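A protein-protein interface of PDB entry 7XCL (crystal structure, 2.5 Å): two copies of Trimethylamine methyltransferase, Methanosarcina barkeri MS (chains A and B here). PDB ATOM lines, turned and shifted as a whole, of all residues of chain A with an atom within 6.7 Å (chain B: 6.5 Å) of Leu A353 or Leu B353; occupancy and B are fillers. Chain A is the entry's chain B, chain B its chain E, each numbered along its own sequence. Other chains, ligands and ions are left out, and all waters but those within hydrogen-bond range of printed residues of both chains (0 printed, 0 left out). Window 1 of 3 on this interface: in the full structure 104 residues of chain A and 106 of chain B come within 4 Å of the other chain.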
ATOM      1  N   LEU A  18       5.692  -0.373 -11.255  1.00  0.00           N
ATOM      2  CA  LEU A  18       4.655   0.247 -12.076  1.00  0.00           C
ATOM      3  C   LEU A  18       3.277  -0.052 -11.472  1.00  0.00           C
ATOM      4  O   LEU A  18       2.889  -1.217 -11.334  1.00  0.00           O
ATOM      5  CB  LEU A  18       4.738  -0.284 -13.516  1.00  0.00           C
ATOM      6  CG  LEU A  18       3.854   0.435 -14.541  1.00  0.00           C
ATOM      7  CD1 LEU A  18       4.552   0.523 -15.867  1.00  0.00           C
ATOM      8  CD2 LEU A  18       2.539  -0.300 -14.686  1.00  0.00           C
ATOM      9  N   TRP A 106       9.672 -14.654 -21.215  1.00  0.00           N
ATOM     10  CA  TRP A 106       9.157 -14.449 -22.568  1.00  0.00           C
ATOM     11  C   TRP A 106       9.059 -15.728 -23.383  1.00  0.00           C
ATOM     12  O   TRP A 106       9.843 -16.659 -23.212  1.00  0.00           O
ATOM     13  CB  TRP A 106      10.043 -13.465 -23.336  1.00  0.00           C
ATOM     14  CG  TRP A 106       9.847 -12.010 -22.999  1.00  0.00           C
ATOM     15  CD1 TRP A 106       9.077 -11.109 -23.675  1.00  0.00           C
ATOM     16  CD2 TRP A 106      10.483 -11.278 -21.943  1.00  0.00           C
ATOM     17  NE1 TRP A 106       9.200  -9.862 -23.115  1.00  0.00           N
ATOM     18  CE2 TRP A 106      10.057  -9.938 -22.049  1.00  0.00           C
ATOM     19  CE3 TRP A 106      11.374 -11.625 -20.919  1.00  0.00           C
ATOM     20  CZ2 TRP A 106      10.495  -8.941 -21.172  1.00  0.00           C
ATOM     21  CZ3 TRP A 106      11.808 -10.635 -20.046  1.00  0.00           C
ATOM     22  CH2 TRP A 106      11.368  -9.308 -20.180  1.00  0.00           C
ATOM     23  N   SER A 333       4.853  -7.497 -26.814  1.00  0.00           N
ATOM     24  CA  SER A 333       5.867  -7.595 -27.853  1.00  0.00           C
ATOM     25  C   SER A 333       5.146  -7.962 -29.144  1.00  0.00           C
ATOM     26  O   SER A 333       5.542  -8.875 -29.863  1.00  0.00           O
ATOM     27  CB  SER A 333       6.902  -8.673 -27.483  1.00  0.00           C
ATOM     28  OG  SER A 333       7.958  -8.723 -28.427  1.00  0.00           O
ATOM     29  N   LYS A 348       6.540  -3.035 -30.589  1.00  0.00           N
ATOM     30  CA  LYS A 348       7.010  -4.192 -29.844  1.00  0.00           C
ATOM     31  C   LYS A 348       7.440  -3.742 -28.463  1.00  0.00           C
ATOM     32  O   LYS A 348       7.175  -4.421 -27.471  1.00  0.00           O
ATOM     33  CB  LYS A 348       8.204  -4.840 -30.556  1.00  0.00           C
ATOM     34  CG  LYS A 348       7.862  -5.579 -31.838  1.00  0.00           C
ATOM     35  CD  LYS A 348       7.196  -6.894 -31.527  1.00  0.00           C
ATOM     36  CE  LYS A 348       6.961  -7.696 -32.784  1.00  0.00           C
ATOM     37  NZ  LYS A 348       6.642  -9.103 -32.431  1.00  0.00           N
ATOM     38  N   THR A 349       8.100  -2.588 -28.417  1.00  0.00           N
ATOM     39  CA  THR A 349       8.612  -2.015 -27.178  1.00  0.00           C
ATOM     40  C   THR A 349       7.486  -1.465 -26.304  1.00  0.00           C
ATOM     41  O   THR A 349       7.480  -1.659 -25.089  1.00  0.00           O
ATOM     42  CB  THR A 349       9.638  -0.892 -27.495  1.00  0.00           C
ATOM     43  OG1 THR A 349      10.635  -1.406 -28.383  1.00  0.00           O
ATOM     44  CG2 THR A 349      10.325  -0.403 -26.224  1.00  0.00           C
ATOM     45  N   MET A 350       6.535  -0.782 -26.929  1.00  0.00           N
ATOM     46  CA  MET A 350       5.393  -0.215 -26.216  1.00  0.00           C
ATOM     47  C   MET A 350       4.585  -1.307 -25.529  1.00  0.00           C
ATOM     48  O   MET A 350       4.202  -1.174 -24.368  1.00  0.00           O
ATOM     49  CB  MET A 350       4.481   0.523 -27.197  1.00  0.00           C
ATOM     50  CG  MET A 350       3.084   0.837 -26.659  1.00  0.00           C
ATOM     51  SD  MET A 350       3.016   2.371 -25.719  1.00  0.00           S
ATOM     52  CE  MET A 350       3.578   1.807 -24.178  1.00  0.00           C
ATOM     53  N   THR A 351       4.337  -2.392 -26.256  1.00  0.00           N
ATOM     54  CA  THR A 351       3.545  -3.502 -25.744  1.00  0.00           C
ATOM     55  C   THR A 351       4.308  -4.519 -24.899  1.00  0.00           C
ATOM     56  O   THR A 351       3.702  -5.395 -24.279  1.00  0.00           O
ATOM     57  CB  THR A 351       2.834  -4.250 -26.905  1.00  0.00           C
ATOM     58  OG1 THR A 351       3.807  -4.890 -27.739  1.00  0.00           O
ATOM     59  CG2 THR A 351       2.030  -3.270 -27.751  1.00  0.00           C
ATOM     60  N   THR A 352       5.632  -4.430 -24.869  1.00  0.00           N
ATOM     61  CA  THR A 352       6.387  -5.382 -24.060  1.00  0.00           C
ATOM     62  C   THR A 352       6.791  -4.729 -22.745  1.00  0.00           C
ATOM     63  O   THR A 352       6.746  -5.354 -21.685  1.00  0.00           O
ATOM     64  CB  THR A 352       7.657  -5.901 -24.790  1.00  0.00           C
ATOM     65  OG1 THR A 352       8.286  -6.914 -23.998  1.00  0.00           O
ATOM     66  CG2 THR A 352       8.646  -4.778 -25.007  1.00  0.00           C
ATOM     67  N   LEU A 353       7.147  -3.453 -22.821  1.00  0.00           N
ATOM     68  CA  LEU A 353       7.587  -2.700 -21.657  1.00  0.00           C
ATOM     69  C   LEU A 353       6.532  -2.550 -20.550  1.00  0.00           C
ATOM     70  O   LEU A 353       6.851  -2.702 -19.365  1.00  0.00           O
ATOM     71  CB  LEU A 353       8.080  -1.330 -22.116  1.00  0.00           C
ATOM     72  CG  LEU A 353       9.122  -0.627 -21.252  1.00  0.00           C
ATOM     73  CD1 LEU A 353      10.264  -1.577 -20.889  1.00  0.00           C
ATOM     74  CD2 LEU A 353       9.638   0.581 -22.025  1.00  0.00           C
ATOM     75  N   LEU A 354       5.285  -2.258 -20.926  1.00  0.00           N
ATOM     76  CA  LEU A 354       4.220  -2.099 -19.934  1.00  0.00           C
ATOM     77  C   LEU A 354       3.961  -3.356 -19.081  1.00  0.00           C
ATOM     78  O   LEU A 354       3.997  -3.292 -17.852  1.00  0.00           O
ATOM     79  CB  LEU A 354       2.927  -1.640 -20.612  1.00  0.00           C
ATOM     80  CG  LEU A 354       2.985  -0.209 -21.158  1.00  0.00           C
ATOM     81  CD1 LEU A 354       1.684   0.152 -21.875  1.00  0.00           C
ATOM     82  CD2 LEU A 354       3.225   0.743 -20.008  1.00  0.00           C
ATOM     83  N   PRO A 355       3.697  -4.509 -19.720  1.00  0.00           N
ATOM     84  CA  PRO A 355       3.445  -5.756 -18.989  1.00  0.00           C
ATOM     85  C   PRO A 355       4.675  -6.193 -18.171  1.00  0.00           C
ATOM     86  O   PRO A 355       4.542  -6.700 -17.058  1.00  0.00           O
ATOM     87  CB  PRO A 355       3.153  -6.762 -20.100  1.00  0.00           C
ATOM     88  CG  PRO A 355       2.734  -5.921 -21.254  1.00  0.00           C
ATOM     89  CD  PRO A 355       3.630  -4.737 -21.173  1.00  0.00           C
ATOM     90  N   ALA A 356       5.864  -6.006 -18.746  1.00  0.00           N
ATOM     91  CA  ALA A 356       7.115  -6.389 -18.106  1.00  0.00           C
ATOM     92  C   ALA A 356       7.342  -5.625 -16.817  1.00  0.00           C
ATOM     93  O   ALA A 356       7.624  -6.225 -15.780  1.00  0.00           O
ATOM     94  CB  ALA A 356       8.291  -6.162 -19.058  1.00  0.00           C
ATOM     95  N   LEU A 357       7.226  -4.302 -16.877  1.00  0.00           N
ATOM     96  CA  LEU A 357       7.414  -3.492 -15.683  1.00  0.00           C
ATOM     97  C   LEU A 357       6.324  -3.822 -14.674  1.00  0.00           C
ATOM     98  O   LEU A 357       6.533  -3.721 -13.464  1.00  0.00           O
ATOM     99  CB  LEU A 357       7.372  -2.007 -16.038  1.00  0.00           C
ATOM    100  CG  LEU A 357       8.539  -1.555 -16.913  1.00  0.00           C
ATOM    101  CD1 LEU A 357       8.436  -0.067 -17.210  1.00  0.00           C
ATOM    102  CD2 LEU A 357       9.842  -1.873 -16.195  1.00  0.00           C
ATOM    103  N   ALA A 358       5.161  -4.224 -15.184  1.00  0.00           N
ATOM    104  CA  ALA A 358       4.026  -4.578 -14.345  1.00  0.00           C
ATOM    105  C   ALA A 358       4.248  -5.917 -13.631  1.00  0.00           C
ATOM    106  O   ALA A 358       3.687  -6.160 -12.560  1.00  0.00           O
ATOM    107  CB  ALA A 358       2.759  -4.637 -15.196  1.00  0.00           C
ATOM    108  N   ILE A 363       5.245 -13.204 -21.217  1.00  0.00           N
ATOM    109  CA  ILE A 363       4.830 -12.221 -22.207  1.00  0.00           C
ATOM    110  C   ILE A 363       5.057 -12.898 -23.546  1.00  0.00           C
ATOM    111  O   ILE A 363       6.185 -13.291 -23.855  1.00  0.00           O
ATOM    112  CB  ILE A 363       5.678 -10.940 -22.132  1.00  0.00           C
ATOM    113  CG1 ILE A 363       5.474 -10.264 -20.770  1.00  0.00           C
ATOM    114  CG2 ILE A 363       5.281  -9.998 -23.264  1.00  0.00           C
ATOM    115  CD1 ILE A 363       6.320  -9.025 -20.553  1.00  0.00           C
ATOM    116  N   MET A 389      17.446  -5.586 -23.508  1.00  0.00           N
ATOM    117  CA  MET A 389      17.452  -4.193 -23.092  1.00  0.00           C
ATOM    118  C   MET A 389      16.424  -3.981 -21.979  1.00  0.00           C
ATOM    119  O   MET A 389      16.662  -3.217 -21.035  1.00  0.00           O
ATOM    120  CB  MET A 389      17.150  -3.294 -24.283  1.00  0.00           C
ATOM    121  CG  MET A 389      18.126  -3.463 -25.431  1.00  0.00           C
ATOM    122  SD  MET A 389      19.832  -3.085 -24.961  1.00  0.00           S
ATOM    123  CE  MET A 389      20.381  -4.672 -24.329  1.00  0.00           C
ATOM    124  N   VAL A 390      15.287  -4.666 -22.077  1.00  0.00           N
ATOM    125  CA  VAL A 390      14.262  -4.546 -21.045  1.00  0.00           C
ATOM    126  C   VAL A 390      14.802  -5.098 -19.719  1.00  0.00           C
ATOM    127  O   VAL A 390      14.559  -4.528 -18.647  1.00  0.00           O
ATOM    128  CB  VAL A 390      12.971  -5.307 -21.433  1.00  0.00           C
ATOM    129  CG1 VAL A 390      11.976  -5.273 -20.286  1.00  0.00           C
ATOM    130  CG2 VAL A 390      12.348  -4.665 -22.659  1.00  0.00           C
ATOM    131  N   ALA A 393      16.756  -2.395 -18.137  1.00  0.00           N
ATOM    132  CA  ALA A 393      15.842  -1.373 -17.651  1.00  0.00           C
ATOM    133  C   ALA A 393      15.177  -1.832 -16.353  1.00  0.00           C
ATOM    134  O   ALA A 393      14.982  -1.040 -15.431  1.00  0.00           O
ATOM    135  CB  ALA A 393      14.787  -1.082 -18.703  1.00  0.00           C
ATOM    136  N   MET A 394      14.839  -3.113 -16.280  1.00  0.00           N
ATOM    137  CA  MET A 394      14.194  -3.645 -15.094  1.00  0.00           C
ATOM    138  C   MET A 394      15.141  -3.717 -13.899  1.00  0.00           C
ATOM    139  O   MET A 394      14.745  -4.076 -12.792  1.00  0.00           O
ATOM    140  CB  MET A 394      13.602  -5.014 -15.402  1.00  0.00           C
ATOM    141  CG  MET A 394      12.398  -4.930 -16.329  1.00  0.00           C
ATOM    142  SD  MET A 394      11.572  -6.506 -16.595  1.00  0.00           S
ATOM    143  CE  MET A 394      11.078  -6.959 -14.881  1.00  0.00           C
ATOM    144  N   LEU B  18       5.184   5.292 -11.916  1.00  0.00           N
ATOM    145  CA  LEU B  18       6.428   4.557 -12.099  1.00  0.00           C
ATOM    146  C   LEU B  18       7.345   4.937 -10.954  1.00  0.00           C
ATOM    147  O   LEU B  18       7.669   6.112 -10.770  1.00  0.00           O
ATOM    148  CB  LEU B  18       7.071   4.898 -13.444  1.00  0.00           C
ATOM    149  CG  LEU B  18       8.274   4.035 -13.838  1.00  0.00           C
ATOM    150  CD1 LEU B  18       8.488   4.103 -15.327  1.00  0.00           C
ATOM    151  CD2 LEU B  18       9.515   4.508 -13.105  1.00  0.00           C
ATOM    152  N   SER B 333      13.414   9.742 -26.154  1.00  0.00           N
ATOM    153  CA  SER B 333      13.059   9.614 -27.555  1.00  0.00           C
ATOM    154  C   SER B 333      14.352   9.781 -28.371  1.00  0.00           C
ATOM    155  O   SER B 333      14.400  10.490 -29.377  1.00  0.00           O
ATOM    156  CB  SER B 333      12.023  10.685 -27.930  1.00  0.00           C
ATOM    157  OG  SER B 333      11.578  10.533 -29.267  1.00  0.00           O
ATOM    158  N   LYS B 348      13.639   4.763 -29.415  1.00  0.00           N
ATOM    159  CA  LYS B 348      12.862   5.973 -29.219  1.00  0.00           C
ATOM    160  C   LYS B 348      11.762   5.713 -28.201  1.00  0.00           C
ATOM    161  O   LYS B 348      11.446   6.573 -27.383  1.00  0.00           O
ATOM    162  CB  LYS B 348      12.231   6.409 -30.534  1.00  0.00           C
ATOM    163  CG  LYS B 348      13.220   6.921 -31.544  1.00  0.00           C
ATOM    164  CD  LYS B 348      13.608   8.334 -31.208  1.00  0.00           C
ATOM    165  CE  LYS B 348      14.633   8.866 -32.185  1.00  0.00           C
ATOM    166  NZ  LYS B 348      14.631  10.355 -32.169  1.00  0.00           N
ATOM    167  N   THR B 349      11.189   4.517 -28.248  1.00  0.00           N
ATOM    168  CA  THR B 349      10.105   4.162 -27.344  1.00  0.00           C
ATOM    169  C   THR B 349      10.639   3.837 -25.952  1.00  0.00           C
ATOM    170  O   THR B 349      10.060   4.248 -24.942  1.00  0.00           O
ATOM    171  CB  THR B 349       9.296   2.960 -27.896  1.00  0.00           C
ATOM    172  OG1 THR B 349       8.918   3.219 -29.255  1.00  0.00           O
ATOM    173  CG2 THR B 349       8.033   2.753 -27.086  1.00  0.00           C
ATOM    174  N   MET B 350      11.747   3.105 -25.905  1.00  0.00           N
ATOM    175  CA  MET B 350      12.377   2.746 -24.638  1.00  0.00           C
ATOM    176  C   MET B 350      12.761   4.007 -23.853  1.00  0.00           C
ATOM    177  O   MET B 350      12.426   4.156 -22.676  1.00  0.00           O
ATOM    178  CB  MET B 350      13.642   1.923 -24.904  1.00  0.00           C
ATOM    179  CG  MET B 350      14.511   1.639 -23.681  1.00  0.00           C
ATOM    180  SD  MET B 350      14.002   0.168 -22.790  1.00  0.00           S
ATOM    181  CE  MET B 350      13.049   0.897 -21.528  1.00  0.00           C
ATOM    182  N   THR B 351      13.451   4.920 -24.526  1.00  0.00           N
ATOM    183  CA  THR B 351      13.930   6.145 -23.904  1.00  0.00           C
ATOM    184  C   THR B 351      12.879   7.228 -23.670  1.00  0.00           C
ATOM    185  O   THR B 351      13.104   8.143 -22.881  1.00  0.00           O
ATOM    186  CB  THR B 351      15.096   6.738 -24.724  1.00  0.00           C
ATOM    187  OG1 THR B 351      14.645   7.035 -26.056  1.00  0.00           O
ATOM    188  CG2 THR B 351      16.254   5.734 -24.794  1.00  0.00           C
ATOM    189  N   THR B 352      11.739   7.154 -24.343  1.00  0.00           N
ATOM    190  CA  THR B 352      10.730   8.171 -24.098  1.00  0.00           C
ATOM    191  C   THR B 352       9.738   7.709 -23.028  1.00  0.00           C
ATOM    192  O   THR B 352       9.284   8.501 -22.197  1.00  0.00           O
ATOM    193  CB  THR B 352       9.962   8.536 -25.383  1.00  0.00           C
ATOM    194  OG1 THR B 352       9.211   9.727 -25.153  1.00  0.00           O
ATOM    195  CG2 THR B 352       9.003   7.444 -25.770  1.00  0.00           C
ATOM    196  N   LEU B 353       9.443   6.412 -23.032  1.00  0.00           N
ATOM    197  CA  LEU B 353       8.481   5.825 -22.104  1.00  0.00           C
ATOM    198  C   LEU B 353       8.891   5.835 -20.626  1.00  0.00           C
ATOM    199  O   LEU B 353       8.088   6.184 -19.760  1.00  0.00           O
ATOM    200  CB  LEU B 353       8.162   4.401 -22.559  1.00  0.00           C
ATOM    201  CG  LEU B 353       6.817   3.776 -22.183  1.00  0.00           C
ATOM    202  CD1 LEU B 353       5.668   4.763 -22.369  1.00  0.00           C
ATOM    203  CD2 LEU B 353       6.619   2.552 -23.064  1.00  0.00           C
ATOM    204  N   LEU B 354      10.127   5.453 -20.326  1.00  0.00           N
ATOM    205  CA  LEU B 354      10.570   5.459 -18.937  1.00  0.00           C
ATOM    206  C   LEU B 354      10.486   6.877 -18.338  1.00  0.00           C
ATOM    207  O   LEU B 354       9.924   7.065 -17.264  1.00  0.00           O
ATOM    208  CB  LEU B 354      11.989   4.882 -18.829  1.00  0.00           C
ATOM    209  CG  LEU B 354      12.070   3.386 -19.168  1.00  0.00           C
ATOM    210  CD1 LEU B 354      13.499   2.887 -19.089  1.00  0.00           C
ATOM    211  CD2 LEU B 354      11.195   2.604 -18.198  1.00  0.00           C
ATOM    212  N   PRO B 355      11.025   7.896 -19.032  1.00  0.00           N
ATOM    213  CA  PRO B 355      10.961   9.270 -18.507  1.00  0.00           C
ATOM    214  C   PRO B 355       9.517   9.800 -18.423  1.00  0.00           C
ATOM    215  O   PRO B 355       9.158  10.500 -17.472  1.00  0.00           O
ATOM    216  CB  PRO B 355      11.777  10.074 -19.521  1.00  0.00           C
ATOM    217  CG  PRO B 355      12.696   9.069 -20.112  1.00  0.00           C
ATOM    218  CD  PRO B 355      11.837   7.843 -20.259  1.00  0.00           C
ATOM    219  N   ALA B 356       8.704   9.476 -19.431  1.00  0.00           N
ATOM    220  CA  ALA B 356       7.315   9.929 -19.486  1.00  0.00           C
ATOM    221  C   ALA B 356       6.485   9.416 -18.322  1.00  0.00           C
ATOM    222  O   ALA B 356       5.822  10.197 -17.633  1.00  0.00           O
ATOM    223  CB  ALA B 356       6.676   9.508 -20.796  1.00  0.00           C
ATOM    224  N   LEU B 357       6.509   8.105 -18.106  1.00  0.00           N
ATOM    225  CA  LEU B 357       5.751   7.531 -17.008  1.00  0.00           C
ATOM    226  C   LEU B 357       6.279   8.079 -15.683  1.00  0.00           C
ATOM    227  O   LEU B 357       5.534   8.186 -14.702  1.00  0.00           O
ATOM    228  CB  LEU B 357       5.856   6.003 -17.035  1.00  0.00           C
ATOM    229  CG  LEU B 357       5.245   5.345 -18.278  1.00  0.00           C
ATOM    230  CD1 LEU B 357       5.460   3.841 -18.239  1.00  0.00           C
ATOM    231  CD2 LEU B 357       3.759   5.680 -18.351  1.00  0.00           C
ATOM    232  N   ALA B 358       7.562   8.442 -15.667  1.00  0.00           N
ATOM    233  CA  ALA B 358       8.196   8.975 -14.462  1.00  0.00           C
ATOM    234  C   ALA B 358       7.730  10.398 -14.162  1.00  0.00           C
ATOM    235  O   ALA B 358       7.684  10.806 -13.001  1.00  0.00           O
ATOM    236  CB  ALA B 358       9.713   8.941 -14.607  1.00  0.00           C
ATOM    237  N   ILE B 363      10.746  16.285 -22.312  1.00  0.00           N
ATOM    238  CA  ILE B 363      11.564  15.203 -22.828  1.00  0.00           C
ATOM    239  C   ILE B 363      12.058  15.658 -24.189  1.00  0.00           C
ATOM    240  O   ILE B 363      11.258  15.854 -25.098  1.00  0.00           O
ATOM    241  CB  ILE B 363      10.745  13.906 -23.001  1.00  0.00           C
ATOM    242  CG1 ILE B 363      10.202  13.447 -21.642  1.00  0.00           C
ATOM    243  CG2 ILE B 363      11.623  12.820 -23.620  1.00  0.00           C
ATOM    244  CD1 ILE B 363       9.200  12.300 -21.731  1.00  0.00           C
ATOM    245  N   VAL B 390       1.990   7.347 -26.443  1.00  0.00           N
ATOM    246  CA  VAL B 390       2.381   7.414 -25.043  1.00  0.00           C
ATOM    247  C   VAL B 390       1.321   8.136 -24.209  1.00  0.00           C
ATOM    248  O   VAL B 390       1.090   7.798 -23.047  1.00  0.00           O
ATOM    249  CB  VAL B 390       3.733   8.142 -24.871  1.00  0.00           C
ATOM    250  CG1 VAL B 390       4.103   8.219 -23.399  1.00  0.00           C
ATOM    251  CG2 VAL B 390       4.806   7.407 -25.634  1.00  0.00           C
ATOM    252  N   ALA B 393      -1.310   5.736 -23.318  1.00  0.00           N
ATOM    253  CA  ALA B 393      -0.797   4.831 -22.314  1.00  0.00           C
ATOM    254  C   ALA B 393      -0.865   5.500 -20.945  1.00  0.00           C
ATOM    255  O   ALA B 393      -1.241   4.867 -19.956  1.00  0.00           O
ATOM    256  CB  ALA B 393       0.637   4.450 -22.640  1.00  0.00           C
ATOM    257  N   MET B 394      -0.514   6.782 -20.887  1.00  0.00           N
ATOM    258  CA  MET B 394      -0.523   7.506 -19.623  1.00  0.00           C
ATOM    259  C   MET B 394      -1.909   7.664 -19.029  1.00  0.00           C
ATOM    260  O   MET B 394      -2.055   8.083 -17.885  1.00  0.00           O
ATOM    261  CB  MET B 394       0.144   8.867 -19.791  1.00  0.00           C
ATOM    262  CG  MET B 394       1.644   8.741 -19.901  1.00  0.00           C
ATOM    263  SD  MET B 394       2.457  10.269 -20.308  1.00  0.00           S
ATOM    264  CE  MET B 394       2.623  11.049 -18.697  1.00  0.00           C
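Among the printed residues, pairs that only touch across the chains: Met A350 with Leu B353 (3.3 Å), Leu A353 with Met B350 (3.5 Å), Leu A353 with Leu B353 (3.8 Å), Thr A349 with Met B350 (3.8 Å), Met A350 with Thr B349 (3.8 Å), Ala A393 with Met B350 (3.9 Å), Thr A349 with Thr B349 (3.9 Å) and Leu A357 with Leu B354 (3.97 Å).
Of chain B, only Met B350 (3.5 Å) and Leu B353 (3.8 Å) come within 4 Å of Leu A353.
Leu B353 touches just these residues of chain A: Met A350 and Leu A353.
Of the printed residues of chain B, Thr A349 touches Thr B349 and Met B350.
Of the printed residues of chain A, Met B350 touches Thr A349 (3.8 Å), Leu A353 (3.5 Å) and Ala A393 (3.9 Å).
Ser A333 touches none of the printed residues of chain B.
The nearest residue of chain B that does not touch Leu A353 is Leu B354 (4.6 Å).
The nearest residue of chain A that does not touch Leu B353 is Thr A349 (4.8 Å).
Of the 19 printed residues of chain A, 5 touch a printed residue of chain B.
Printed residues of chain B that touch a printed residue of chain A: Thr B349, Met B350, Leu B353 and Leu B354.
Hydrophobic or aromatic side chains of chain B that line the printed part of chain A: Met B350, Leu B353 and Leu B354.
Among the printed residues, 8 pairs touch across the chains.
Thr B349 touches its own counterpart, Thr A349.
Thr A349 touches Met B350, and with the chains exchanged Met A350 touches Thr B349.
Leu B353 touches its own counterpart, Leu A353.
Leu A357 touches Leu B354, but with the chains exchanged Leu A354 does not touch Leu B357 (4.2 Å).
17 positions are printed for both chains.
Of the 8 pairs that touch across the chains among the printed residues, 6 have their exchanged pair printed and touching as well.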
